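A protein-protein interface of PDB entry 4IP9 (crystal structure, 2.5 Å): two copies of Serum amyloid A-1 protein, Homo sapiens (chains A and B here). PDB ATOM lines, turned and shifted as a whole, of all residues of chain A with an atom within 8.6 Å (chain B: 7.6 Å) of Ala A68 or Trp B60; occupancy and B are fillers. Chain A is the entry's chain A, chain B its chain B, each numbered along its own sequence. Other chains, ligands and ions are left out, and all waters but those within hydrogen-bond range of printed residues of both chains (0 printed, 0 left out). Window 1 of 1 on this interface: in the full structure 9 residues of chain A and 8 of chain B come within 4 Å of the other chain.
ND2 of Asn A71 is in hydrogen-bond range of O of Asp A67. The side-chain amide oxygen (OD1) of Asn A71 is in hydrogen-bond range of the guanidinium group (NH1) of Arg A74 (2.8 Å).
Of the 21 printed residues of chain B, 3 touch a printed residue of chain A. Of the 18 printed residues of chain A, 5 touch a printed residue of chain B. Hydrophobic or aromatic side chains of chain A within 4 Å of the printed part of chain B: Ala A68, Ile A72, Phe A75 and Phe A76. Among the printed residues, no Asp or Glu carboxylate lies within 4 Å of a Lys or Arg side-chain nitrogen of the other chain.
Of the printed residues of chain B, Ala A68 touches Trp B60 (2.8 Å). Glu A70 touches none of the printed residues of chain B. Printed residues of chain B within 4 Å of Asn A71: Trp B60 (3.8 Å). Of the printed residues of chain B, Ile A72 touches Phe B13 (3.4 Å) and Trp B60 (3.5 Å). Of the printed residues of chain B, Phe A76 touches Phe B13 (3.6 Å). Printed residues of chain A within 4 Å of Pro B56: Phe A75. No residue of chain A comes within 4 Å of Gly B58. Val B59 touches none of the printed residues of chain A. Trp B60 touches three residues of chain A. No residue of chain A comes within 4 Å of Ala B61. The nearest residue of chain A that does not touch Trp B60 is Arg A69 (4.8 Å).
The indole nitrogen (NE1) of Trp B60 sits at hydrogen-bond distance from the backbone carbonyl oxygen (O) of Ala A68 (2.8 Å).
Among the printed residues, pairs that only touch across the chains: Ile A72 with Phe B13 (3.4 Å), Ile A72 with Trp B60 (3.5 Å), Phe A75 with Phe B13 (3.5 Å), Phe A76 with Phe B13 (3.6 Å), Phe A75 with Pro B56 (3.6 Å) and Asn A71 with Trp B60 (3.8 Å).
Positions printed for both chains: 61, 62, 63, 64, 65, 66, 67 and 94. Of the 7 pairs that touch across the chains among the printed residues, none has its exchanged pair printed and touching as well.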
ATOM      1  N   ALA A  61      -0.631  13.032 -35.610  1.00  0.00           N
ATOM      2  CA  ALA A  61       0.678  13.083 -34.942  1.00  0.00           C
ATOM      3  C   ALA A  61       1.620  14.112 -35.590  1.00  0.00           C
ATOM      4  O   ALA A  61       2.247  14.881 -34.863  1.00  0.00           O
ATOM      5  CB  ALA A  61       1.320  11.708 -34.924  1.00  0.00           C
ATOM      6  N   ALA A  62       1.666  14.179 -36.941  1.00  0.00           N
ATOM      7  CA  ALA A  62       2.482  15.157 -37.683  1.00  0.00           C
ATOM      8  C   ALA A  62       2.074  16.589 -37.346  1.00  0.00           C
ATOM      9  O   ALA A  62       2.946  17.429 -37.122  1.00  0.00           O
ATOM     10  CB  ALA A  62       2.376  14.925 -39.178  1.00  0.00           C
ATOM     11  N   GLU A  63       0.752  16.854 -37.281  1.00  0.00           N
ATOM     12  CA  GLU A  63       0.191  18.162 -36.967  1.00  0.00           C
ATOM     13  C   GLU A  63       0.434  18.526 -35.506  1.00  0.00           C
ATOM     14  O   GLU A  63       0.799  19.664 -35.216  1.00  0.00           O
ATOM     15  CB  GLU A  63      -1.296  18.197 -37.304  1.00  0.00           C
ATOM     16  CG  GLU A  63      -1.927  19.563 -37.102  1.00  0.00           C
ATOM     17  CD  GLU A  63      -3.355  19.712 -37.580  1.00  0.00           C
ATOM     18  OE1 GLU A  63      -4.011  18.686 -37.885  1.00  0.00           O
ATOM     19  OE2 GLU A  63      -3.810  20.875 -37.672  1.00  0.00           O
ATOM     20  N   ALA A  64       0.250  17.565 -34.594  1.00  0.00           N
ATOM     21  CA  ALA A  64       0.492  17.785 -33.180  1.00  0.00           C
ATOM     22  C   ALA A  64       1.970  18.151 -32.980  1.00  0.00           C
ATOM     23  O   ALA A  64       2.256  19.194 -32.388  1.00  0.00           O
ATOM     24  CB  ALA A  64       0.111  16.546 -32.375  1.00  0.00           C
ATOM     25  N   ILE A  65       2.891  17.366 -33.572  1.00  0.00           N
ATOM     26  CA  ILE A  65       4.338  17.613 -33.508  1.00  0.00           C
ATOM     27  C   ILE A  65       4.765  18.938 -34.182  1.00  0.00           C
ATOM     28  O   ILE A  65       5.539  19.684 -33.582  1.00  0.00           O
ATOM     29  CB  ILE A  65       5.150  16.371 -33.970  1.00  0.00           C
ATOM     30  CG1 ILE A  65       4.935  15.198 -32.968  1.00  0.00           C
ATOM     31  CG2 ILE A  65       6.655  16.698 -34.128  1.00  0.00           C
ATOM     32  CD1 ILE A  65       5.146  13.831 -33.577  1.00  0.00           C
ATOM     33  N   SER A  66       4.255  19.230 -35.399  1.00  0.00           N
ATOM     34  CA  SER A  66       4.577  20.461 -36.134  1.00  0.00           C
ATOM     35  C   SER A  66       4.131  21.719 -35.383  1.00  0.00           C
ATOM     36  O   SER A  66       4.913  22.664 -35.298  1.00  0.00           O
ATOM     37  CB  SER A  66       3.974  20.453 -37.537  1.00  0.00           C
ATOM     38  OG  SER A  66       4.507  19.395 -38.315  1.00  0.00           O
ATOM     39  N   ASP A  67       2.894  21.727 -34.833  1.00  0.00           N
ATOM     40  CA  ASP A  67       2.372  22.862 -34.074  1.00  0.00           C
ATOM     41  C   ASP A  67       3.210  23.124 -32.818  1.00  0.00           C
ATOM     42  O   ASP A  67       3.558  24.284 -32.565  1.00  0.00           O
ATOM     43  CB  ASP A  67       0.888  22.667 -33.703  1.00  0.00           C
ATOM     44  CG  ASP A  67      -0.097  22.731 -34.860  1.00  0.00           C
ATOM     45  OD1 ASP A  67       0.215  23.401 -35.879  1.00  0.00           O
ATOM     46  OD2 ASP A  67      -1.193  22.155 -34.731  1.00  0.00           O
ATOM     47  N   ALA A  68       3.564  22.055 -32.055  1.00  0.00           N
ATOM     48  CA  ALA A  68       4.380  22.186 -30.838  1.00  0.00           C
ATOM     49  C   ALA A  68       5.784  22.725 -31.134  1.00  0.00           C
ATOM     50  O   ALA A  68       6.266  23.602 -30.408  1.00  0.00           O
ATOM     51  CB  ALA A  68       4.466  20.860 -30.097  1.00  0.00           C
ATOM     52  N   ARG A  69       6.408  22.243 -32.227  1.00  0.00           N
ATOM     53  CA  ARG A  69       7.740  22.649 -32.665  1.00  0.00           C
ATOM     54  C   ARG A  69       7.758  24.139 -33.012  1.00  0.00           C
ATOM     55  O   ARG A  69       8.636  24.876 -32.566  1.00  0.00           O
ATOM     56  CB  ARG A  69       8.157  21.812 -33.873  1.00  0.00           C
ATOM     57  CG  ARG A  69       9.667  21.784 -34.125  1.00  0.00           C
ATOM     58  CD  ARG A  69      10.052  22.261 -35.513  1.00  0.00           C
ATOM     59  NE  ARG A  69       9.204  21.682 -36.554  1.00  0.00           N
ATOM     60  CZ  ARG A  69       8.401  22.383 -37.343  1.00  0.00           C
ATOM     61  NH1 ARG A  69       8.344  23.704 -37.240  1.00  0.00           N
ATOM     62  NH2 ARG A  69       7.651  21.771 -38.243  1.00  0.00           N
ATOM     63  N   GLU A  70       6.760  24.577 -33.786  1.00  0.00           N
ATOM     64  CA  GLU A  70       6.559  25.949 -34.218  1.00  0.00           C
ATOM     65  C   GLU A  70       6.403  26.879 -33.001  1.00  0.00           C
ATOM     66  O   GLU A  70       6.994  27.967 -32.984  1.00  0.00           O
ATOM     67  CB  GLU A  70       5.317  25.983 -35.119  1.00  0.00           C
ATOM     68  CG  GLU A  70       4.884  27.342 -35.641  1.00  0.00           C
ATOM     69  CD  GLU A  70       3.430  27.333 -36.072  1.00  0.00           C
ATOM     70  OE1 GLU A  70       2.739  28.354 -35.849  1.00  0.00           O
ATOM     71  OE2 GLU A  70       2.968  26.298 -36.608  1.00  0.00           O
ATOM     72  N   ASN A  71       5.627  26.442 -31.988  1.00  0.00           N
ATOM     73  CA  ASN A  71       5.371  27.208 -30.764  1.00  0.00           C
ATOM     74  C   ASN A  71       6.581  27.319 -29.835  1.00  0.00           C
ATOM     75  O   ASN A  71       6.802  28.383 -29.240  1.00  0.00           O
ATOM     76  CB  ASN A  71       4.138  26.678 -30.030  1.00  0.00           C
ATOM     77  CG  ASN A  71       2.844  27.207 -30.602  1.00  0.00           C
ATOM     78  OD1 ASN A  71       2.431  28.337 -30.312  1.00  0.00           O
ATOM     79  ND2 ASN A  71       2.198  26.427 -31.460  1.00  0.00           N
ATOM     80  N   ILE A  72       7.363  26.232 -29.719  1.00  0.00           N
ATOM     81  CA  ILE A  72       8.569  26.200 -28.895  1.00  0.00           C
ATOM     82  C   ILE A  72       9.645  27.126 -29.502  1.00  0.00           C
ATOM     83  O   ILE A  72      10.205  27.969 -28.786  1.00  0.00           O
ATOM     84  CB  ILE A  72       9.035  24.755 -28.531  1.00  0.00           C
ATOM     85  CG1 ILE A  72      10.024  24.743 -27.351  1.00  0.00           C
ATOM     86  CG2 ILE A  72       9.585  23.974 -29.725  1.00  0.00           C
ATOM     87  CD1 ILE A  72      10.142  23.372 -26.648  1.00  0.00           C
ATOM     88  N   GLN A  73       9.822  27.055 -30.848  1.00  0.00           N
ATOM     89  CA  GLN A  73      10.763  27.899 -31.611  1.00  0.00           C
ATOM     90  C   GLN A  73      10.397  29.382 -31.463  1.00  0.00           C
ATOM     91  O   GLN A  73      11.280  30.223 -31.272  1.00  0.00           O
ATOM     92  CB  GLN A  73      10.815  27.489 -33.102  1.00  0.00           C
ATOM     93  CG  GLN A  73      11.581  26.176 -33.391  1.00  0.00           C
ATOM     94  CD  GLN A  73      11.844  25.990 -34.878  1.00  0.00           C
ATOM     95  OE1 GLN A  73      11.103  25.300 -35.587  1.00  0.00           O
ATOM     96  NE2 GLN A  73      12.887  26.638 -35.398  1.00  0.00           N
ATOM     97  N   ARG A  74       9.089  29.682 -31.492  1.00  0.00           N
ATOM     98  CA  ARG A  74       8.561  31.032 -31.331  1.00  0.00           C
ATOM     99  C   ARG A  74       8.930  31.633 -29.964  1.00  0.00           C
ATOM    100  O   ARG A  74       9.362  32.789 -29.909  1.00  0.00           O
ATOM    101  CB  ARG A  74       7.039  31.049 -31.540  1.00  0.00           C
ATOM    102  CG  ARG A  74       6.493  32.446 -31.820  1.00  0.00           C
ATOM    103  CD  ARG A  74       4.979  32.498 -31.808  1.00  0.00           C
ATOM    104  NE  ARG A  74       4.406  31.998 -33.057  1.00  0.00           N
ATOM    105  CZ  ARG A  74       3.821  30.815 -33.197  1.00  0.00           C
ATOM    106  NH1 ARG A  74       3.698  30.001 -32.156  1.00  0.00           N
ATOM    107  NH2 ARG A  74       3.325  30.451 -34.368  1.00  0.00           N
ATOM    108  N   PHE A  75       8.774  30.847 -28.875  1.00  0.00           N
ATOM    109  CA  PHE A  75       9.084  31.283 -27.509  1.00  0.00           C
ATOM    110  C   PHE A  75      10.567  31.632 -27.307  1.00  0.00           C
ATOM    111  O   PHE A  75      10.877  32.600 -26.609  1.00  0.00           O
ATOM    112  CB  PHE A  75       8.614  30.235 -26.468  1.00  0.00           C
ATOM    113  CG  PHE A  75       9.056  30.522 -25.046  1.00  0.00           C
ATOM    114  CD1 PHE A  75       8.346  31.410 -24.244  1.00  0.00           C
ATOM    115  CD2 PHE A  75      10.212  29.943 -24.529  1.00  0.00           C
ATOM    116  CE1 PHE A  75       8.774  31.698 -22.945  1.00  0.00           C
ATOM    117  CE2 PHE A  75      10.639  30.234 -23.231  1.00  0.00           C
ATOM    118  CZ  PHE A  75       9.913  31.101 -22.446  1.00  0.00           C
ATOM    119  N   PHE A  76      11.470  30.824 -27.879  1.00  0.00           N
ATOM    120  CA  PHE A  76      12.908  31.018 -27.717  1.00  0.00           C
ATOM    121  C   PHE A  76      13.572  32.138 -28.526  1.00  0.00           C
ATOM    122  O   PHE A  76      14.581  32.680 -28.070  1.00  0.00           O
ATOM    123  CB  PHE A  76      13.677  29.688 -27.745  1.00  0.00           C
ATOM    124  CG  PHE A  76      13.444  28.837 -26.515  1.00  0.00           C
ATOM    125  CD1 PHE A  76      14.022  29.173 -25.295  1.00  0.00           C
ATOM    126  CD2 PHE A  76      12.651  27.701 -26.576  1.00  0.00           C
ATOM    127  CE1 PHE A  76      13.799  28.391 -24.157  1.00  0.00           C
ATOM    128  CE2 PHE A  76      12.441  26.913 -25.440  1.00  0.00           C
ATOM    129  CZ  PHE A  76      13.018  27.261 -24.241  1.00  0.00           C
ATOM    130  N   ASN A  90       5.400  22.164 -43.826  1.00  0.00           N
ATOM    131  CA  ASN A  90       4.709  21.098 -43.081  1.00  0.00           C
ATOM    132  C   ASN A  90       3.392  20.695 -43.768  1.00  0.00           C
ATOM    133  O   ASN A  90       3.143  19.502 -43.952  1.00  0.00           O
ATOM    134  CB  ASN A  90       4.412  21.531 -41.632  1.00  0.00           C
ATOM    135  CG  ASN A  90       5.605  21.726 -40.730  1.00  0.00           C
ATOM    136  OD1 ASN A  90       5.639  22.650 -39.920  1.00  0.00           O
ATOM    137  ND2 ASN A  90       6.583  20.851 -40.788  1.00  0.00           N
ATOM    138  N   ARG A  94       2.235  16.921 -45.379  1.00  0.00           N
ATOM    139  CA  ARG A  94       1.046  16.348 -44.733  1.00  0.00           C
ATOM    140  C   ARG A  94      -0.114  16.115 -45.705  1.00  0.00           C
ATOM    141  O   ARG A  94      -0.837  15.133 -45.560  1.00  0.00           O
ATOM    142  CB  ARG A  94       0.587  17.234 -43.576  1.00  0.00           C
ATOM    143  CG  ARG A  94      -0.058  16.457 -42.445  1.00  0.00           C
ATOM    144  CD  ARG A  94      -0.470  17.366 -41.303  1.00  0.00           C
ATOM    145  NE  ARG A  94       0.667  18.115 -40.772  1.00  0.00           N
ATOM    146  CZ  ARG A  94       0.641  19.411 -40.483  1.00  0.00           C
ATOM    147  NH1 ARG A  94      -0.474  20.111 -40.646  1.00  0.00           N
ATOM    148  NH2 ARG A  94       1.724  20.012 -40.016  1.00  0.00           N
ATOM    149  N   PHE B  13      12.463  24.846 -18.944  1.00  0.00           N
ATOM    150  CA  PHE B  13      11.338  24.824 -19.885  1.00  0.00           C
ATOM    151  C   PHE B  13      10.876  23.374 -20.161  1.00  0.00           C
ATOM    152  O   PHE B  13       9.677  23.115 -20.181  1.00  0.00           O
ATOM    153  CB  PHE B  13      11.730  25.514 -21.203  1.00  0.00           C
ATOM    154  CG  PHE B  13      10.566  25.753 -22.138  1.00  0.00           C
ATOM    155  CD1 PHE B  13       9.827  26.933 -22.068  1.00  0.00           C
ATOM    156  CD2 PHE B  13      10.181  24.784 -23.065  1.00  0.00           C
ATOM    157  CE1 PHE B  13       8.745  27.153 -22.929  1.00  0.00           C
ATOM    158  CE2 PHE B  13       9.079  24.998 -23.908  1.00  0.00           C
ATOM    159  CZ  PHE B  13       8.378  26.186 -23.843  1.00  0.00           C
ATOM    160  N   LEU B  14      11.832  22.431 -20.343  1.00  0.00           N
ATOM    161  CA  LEU B  14      11.515  21.023 -20.584  1.00  0.00           C
ATOM    162  C   LEU B  14      10.952  20.323 -19.363  1.00  0.00           C
ATOM    163  O   LEU B  14       9.998  19.563 -19.497  1.00  0.00           O
ATOM    164  CB  LEU B  14      12.689  20.256 -21.178  1.00  0.00           C
ATOM    165  CG  LEU B  14      13.031  20.561 -22.637  1.00  0.00           C
ATOM    166  CD1 LEU B  14      13.925  19.508 -23.174  1.00  0.00           C
ATOM    167  CD2 LEU B  14      11.774  20.632 -23.522  1.00  0.00           C
ATOM    168  N   GLU B  16       9.374  21.907 -16.893  1.00  0.00           N
ATOM    169  CA  GLU B  16       8.044  22.535 -16.776  1.00  0.00           C
ATOM    170  C   GLU B  16       7.065  21.835 -17.740  1.00  0.00           C
ATOM    171  O   GLU B  16       5.918  21.610 -17.379  1.00  0.00           O
ATOM    172  CB  GLU B  16       8.096  24.042 -17.128  1.00  0.00           C
ATOM    173  CG  GLU B  16       8.884  24.929 -16.176  1.00  0.00           C
ATOM    174  CD  GLU B  16       9.259  26.314 -16.683  1.00  0.00           C
ATOM    175  OE1 GLU B  16       9.047  26.609 -17.883  1.00  0.00           O
ATOM    176  OE2 GLU B  16       9.799  27.101 -15.875  1.00  0.00           O
ATOM    177  N   ALA B  17       7.527  21.485 -18.951  1.00  0.00           N
ATOM    178  CA  ALA B  17       6.713  20.820 -19.967  1.00  0.00           C
ATOM    179  C   ALA B  17       6.280  19.406 -19.537  1.00  0.00           C
ATOM    180  O   ALA B  17       5.080  19.130 -19.532  1.00  0.00           O
ATOM    181  CB  ALA B  17       7.449  20.792 -21.301  1.00  0.00           C
ATOM    182  N   PHE B  18       7.229  18.548 -19.100  1.00  0.00           N
ATOM    183  CA  PHE B  18       6.913  17.200 -18.612  1.00  0.00           C
ATOM    184  C   PHE B  18       5.973  17.249 -17.406  1.00  0.00           C
ATOM    185  O   PHE B  18       5.027  16.470 -17.336  1.00  0.00           O
ATOM    186  CB  PHE B  18       8.187  16.408 -18.286  1.00  0.00           C
ATOM    187  CG  PHE B  18       8.913  15.862 -19.492  1.00  0.00           C
ATOM    188  CD1 PHE B  18       8.457  14.716 -20.144  1.00  0.00           C
ATOM    189  CD2 PHE B  18      10.069  16.479 -19.969  1.00  0.00           C
ATOM    190  CE1 PHE B  18       9.147  14.203 -21.258  1.00  0.00           C
ATOM    191  CE2 PHE B  18      10.771  15.949 -21.064  1.00  0.00           C
ATOM    192  CZ  PHE B  18      10.300  14.823 -21.705  1.00  0.00           C
ATOM    193  N   ALA B  51      -0.857  23.122 -15.267  1.00  0.00           N
ATOM    194  CA  ALA B  51       0.260  23.067 -16.218  1.00  0.00           C
ATOM    195  C   ALA B  51       0.843  24.469 -16.427  1.00  0.00           C
ATOM    196  O   ALA B  51       2.052  24.632 -16.296  1.00  0.00           O
ATOM    197  CB  ALA B  51      -0.193  22.473 -17.541  1.00  0.00           C
ATOM    198  N   ALA B  52      -0.015  25.490 -16.661  1.00  0.00           N
ATOM    199  CA  ALA B  52       0.425  26.875 -16.854  1.00  0.00           C
ATOM    200  C   ALA B  52       1.193  27.417 -15.644  1.00  0.00           C
ATOM    201  O   ALA B  52       2.124  28.204 -15.826  1.00  0.00           O
ATOM    202  CB  ALA B  52      -0.761  27.780 -17.173  1.00  0.00           C
ATOM    203  N   GLY B  55       5.120  27.047 -15.313  1.00  0.00           N
ATOM    204  CA  GLY B  55       5.871  28.044 -16.064  1.00  0.00           C
ATOM    205  C   GLY B  55       5.619  27.977 -17.560  1.00  0.00           C
ATOM    206  O   GLY B  55       4.715  27.265 -18.005  1.00  0.00           O
ATOM    207  N   PRO B  56       6.446  28.681 -18.364  1.00  0.00           N
ATOM    208  CA  PRO B  56       6.270  28.664 -19.830  1.00  0.00           C
ATOM    209  C   PRO B  56       6.218  27.296 -20.510  1.00  0.00           C
ATOM    210  O   PRO B  56       5.459  27.133 -21.464  1.00  0.00           O
ATOM    211  CB  PRO B  56       7.445  29.495 -20.327  1.00  0.00           C
ATOM    212  CG  PRO B  56       7.741  30.402 -19.210  1.00  0.00           C
ATOM    213  CD  PRO B  56       7.549  29.582 -17.981  1.00  0.00           C
ATOM    214  N   GLY B  57       7.007  26.336 -20.023  1.00  0.00           N
ATOM    215  CA  GLY B  57       7.023  24.977 -20.554  1.00  0.00           C
ATOM    216  C   GLY B  57       5.691  24.295 -20.349  1.00  0.00           C
ATOM    217  O   GLY B  57       5.215  23.575 -21.230  1.00  0.00           O
ATOM    218  N   GLY B  58       5.074  24.579 -19.200  1.00  0.00           N
ATOM    219  CA  GLY B  58       3.761  24.083 -18.825  1.00  0.00           C
ATOM    220  C   GLY B  58       2.665  24.643 -19.713  1.00  0.00           C
ATOM    221  O   GLY B  58       1.775  23.893 -20.126  1.00  0.00           O
ATOM    222  N   VAL B  59       2.738  25.955 -20.042  1.00  0.00           N
ATOM    223  CA  VAL B  59       1.793  26.646 -20.933  1.00  0.00           C
ATOM    224  C   VAL B  59       1.842  25.961 -22.312  1.00  0.00           C
ATOM    225  O   VAL B  59       0.803  25.607 -22.865  1.00  0.00           O
ATOM    226  CB  VAL B  59       2.111  28.180 -21.042  1.00  0.00           C
ATOM    227  CG1 VAL B  59       1.337  28.838 -22.182  1.00  0.00           C
ATOM    228  CG2 VAL B  59       1.838  28.906 -19.727  1.00  0.00           C
ATOM    229  N   TRP B  60       3.068  25.781 -22.843  1.00  0.00           N
ATOM    230  CA  TRP B  60       3.358  25.140 -24.124  1.00  0.00           C
ATOM    231  C   TRP B  60       2.796  23.689 -24.172  1.00  0.00           C
ATOM    232  O   TRP B  60       2.067  23.345 -25.106  1.00  0.00           O
ATOM    233  CB  TRP B  60       4.875  25.171 -24.376  1.00  0.00           C
ATOM    234  CG  TRP B  60       5.325  24.416 -25.592  1.00  0.00           C
ATOM    235  CD1 TRP B  60       5.194  24.798 -26.892  1.00  0.00           C
ATOM    236  CD2 TRP B  60       5.980  23.147 -25.612  1.00  0.00           C
ATOM    237  NE1 TRP B  60       5.706  23.836 -27.723  1.00  0.00           N
ATOM    238  CE2 TRP B  60       6.192  22.805 -26.965  1.00  0.00           C
ATOM    239  CE3 TRP B  60       6.399  22.252 -24.614  1.00  0.00           C
ATOM    240  CZ2 TRP B  60       6.849  21.627 -27.347  1.00  0.00           C
ATOM    241  CZ3 TRP B  60       6.992  21.060 -24.991  1.00  0.00           C
ATOM    242  CH2 TRP B  60       7.220  20.759 -26.343  1.00  0.00           C
ATOM    243  N   ALA B  61       3.107  22.879 -23.144  1.00  0.00           N
ATOM    244  CA  ALA B  61       2.652  21.494 -23.017  1.00  0.00           C
ATOM    245  C   ALA B  61       1.119  21.391 -22.918  1.00  0.00           C
ATOM    246  O   ALA B  61       0.535  20.553 -23.601  1.00  0.00           O
ATOM    247  CB  ALA B  61       3.320  20.833 -21.820  1.00  0.00           C
ATOM    248  N   ALA B  62       0.469  22.280 -22.128  1.00  0.00           N
ATOM    249  CA  ALA B  62      -1.000  22.322 -21.988  1.00  0.00           C
ATOM    250  C   ALA B  62      -1.679  22.584 -23.329  1.00  0.00           C
ATOM    251  O   ALA B  62      -2.658  21.914 -23.657  1.00  0.00           O
ATOM    252  CB  ALA B  62      -1.414  23.388 -20.981  1.00  0.00           C
ATOM    253  N   GLU B  63      -1.137  23.537 -24.110  1.00  0.00           N
ATOM    254  CA  GLU B  63      -1.654  23.926 -25.422  1.00  0.00           C
ATOM    255  C   GLU B  63      -1.423  22.826 -26.446  1.00  0.00           C
ATOM    256  O   GLU B  63      -2.330  22.537 -27.230  1.00  0.00           O
ATOM    257  CB  GLU B  63      -1.021  25.243 -25.876  1.00  0.00           C
ATOM    258  CG  GLU B  63      -1.586  25.759 -27.188  1.00  0.00           C
ATOM    259  CD  GLU B  63      -1.128  27.136 -27.609  1.00  0.00           C
ATOM    260  OE1 GLU B  63      -0.152  27.657 -27.024  1.00  0.00           O
ATOM    261  OE2 GLU B  63      -1.752  27.694 -28.537  1.00  0.00           O
ATOM    262  N   ALA B  64      -0.226  22.204 -26.428  1.00  0.00           N
ATOM    263  CA  ALA B  64       0.084  21.088 -27.321  1.00  0.00           C
ATOM    264  C   ALA B  64      -0.898  19.942 -27.054  1.00  0.00           C
ATOM    265  O   ALA B  64      -1.560  19.488 -27.985  1.00  0.00           O
ATOM    266  CB  ALA B  64       1.523  20.623 -27.124  1.00  0.00           C
ATOM    267  N   ILE B  65      -1.071  19.564 -25.780  1.00  0.00           N
ATOM    268  CA  ILE B  65      -1.994  18.500 -25.374  1.00  0.00           C
ATOM    269  C   ILE B  65      -3.484  18.837 -25.673  1.00  0.00           C
ATOM    270  O   ILE B  65      -4.190  17.985 -26.216  1.00  0.00           O
ATOM    271  CB  ILE B  65      -1.726  18.040 -23.905  1.00  0.00           C
ATOM    272  CG1 ILE B  65      -0.336  17.371 -23.797  1.00  0.00           C
ATOM    273  CG2 ILE B  65      -2.821  17.090 -23.387  1.00  0.00           C
ATOM    274  CD1 ILE B  65       0.283  17.438 -22.396  1.00  0.00           C
ATOM    275  N   SER B  66      -3.938  20.069 -25.350  1.00  0.00           N
ATOM    276  CA  SER B  66      -5.323  20.501 -25.597  1.00  0.00           C
ATOM    277  C   SER B  66      -5.683  20.508 -27.080  1.00  0.00           C
ATOM    278  O   SER B  66      -6.758  20.017 -27.434  1.00  0.00           O
ATOM    279  CB  SER B  66      -5.600  21.871 -24.986  1.00  0.00           C
ATOM    280  OG  SER B  66      -5.450  21.854 -23.578  1.00  0.00           O
ATOM    281  N   ASP B  67      -4.791  21.045 -27.942  1.00  0.00           N
ATOM    282  CA  ASP B  67      -5.004  21.076 -29.395  1.00  0.00           C
ATOM    283  C   ASP B  67      -5.102  19.669 -29.975  1.00  0.00           C
ATOM    284  O   ASP B  67      -6.013  19.416 -30.763  1.00  0.00           O
ATOM    285  CB  ASP B  67      -3.906  21.882 -30.121  1.00  0.00           C
ATOM    286  CG  ASP B  67      -3.914  23.384 -29.886  1.00  0.00           C
ATOM    287  OD1 ASP B  67      -5.003  23.945 -29.596  1.00  0.00           O
ATOM    288  OD2 ASP B  67      -2.850  24.010 -30.048  1.00  0.00           O
ATOM    289  N   ARG B  94      -5.485  27.996 -18.661  1.00  0.00           N
ATOM    290  CA  ARG B  94      -4.158  28.350 -19.171  1.00  0.00           C
ATOM    291  C   ARG B  94      -3.809  29.823 -18.942  1.00  0.00           C
ATOM    292  O   ARG B  94      -2.647  30.133 -18.676  1.00  0.00           O
ATOM    293  CB  ARG B  94      -4.046  28.006 -20.654  1.00  0.00           C
ATOM    294  CG  ARG B  94      -2.645  27.582 -21.074  1.00  0.00           C
ATOM    295  CD  ARG B  94      -2.582  27.204 -22.540  1.00  0.00           C
ATOM    296  NE  ARG B  94      -3.517  26.125 -22.871  1.00  0.00           N
ATOM    297  CZ  ARG B  94      -4.312  26.129 -23.934  1.00  0.00           C
ATOM    298  NH1 ARG B  94      -4.285  27.146 -24.787  1.00  0.00           N
ATOM    299  NH2 ARG B  94      -5.130  25.110 -24.162  1.00  0.00           N
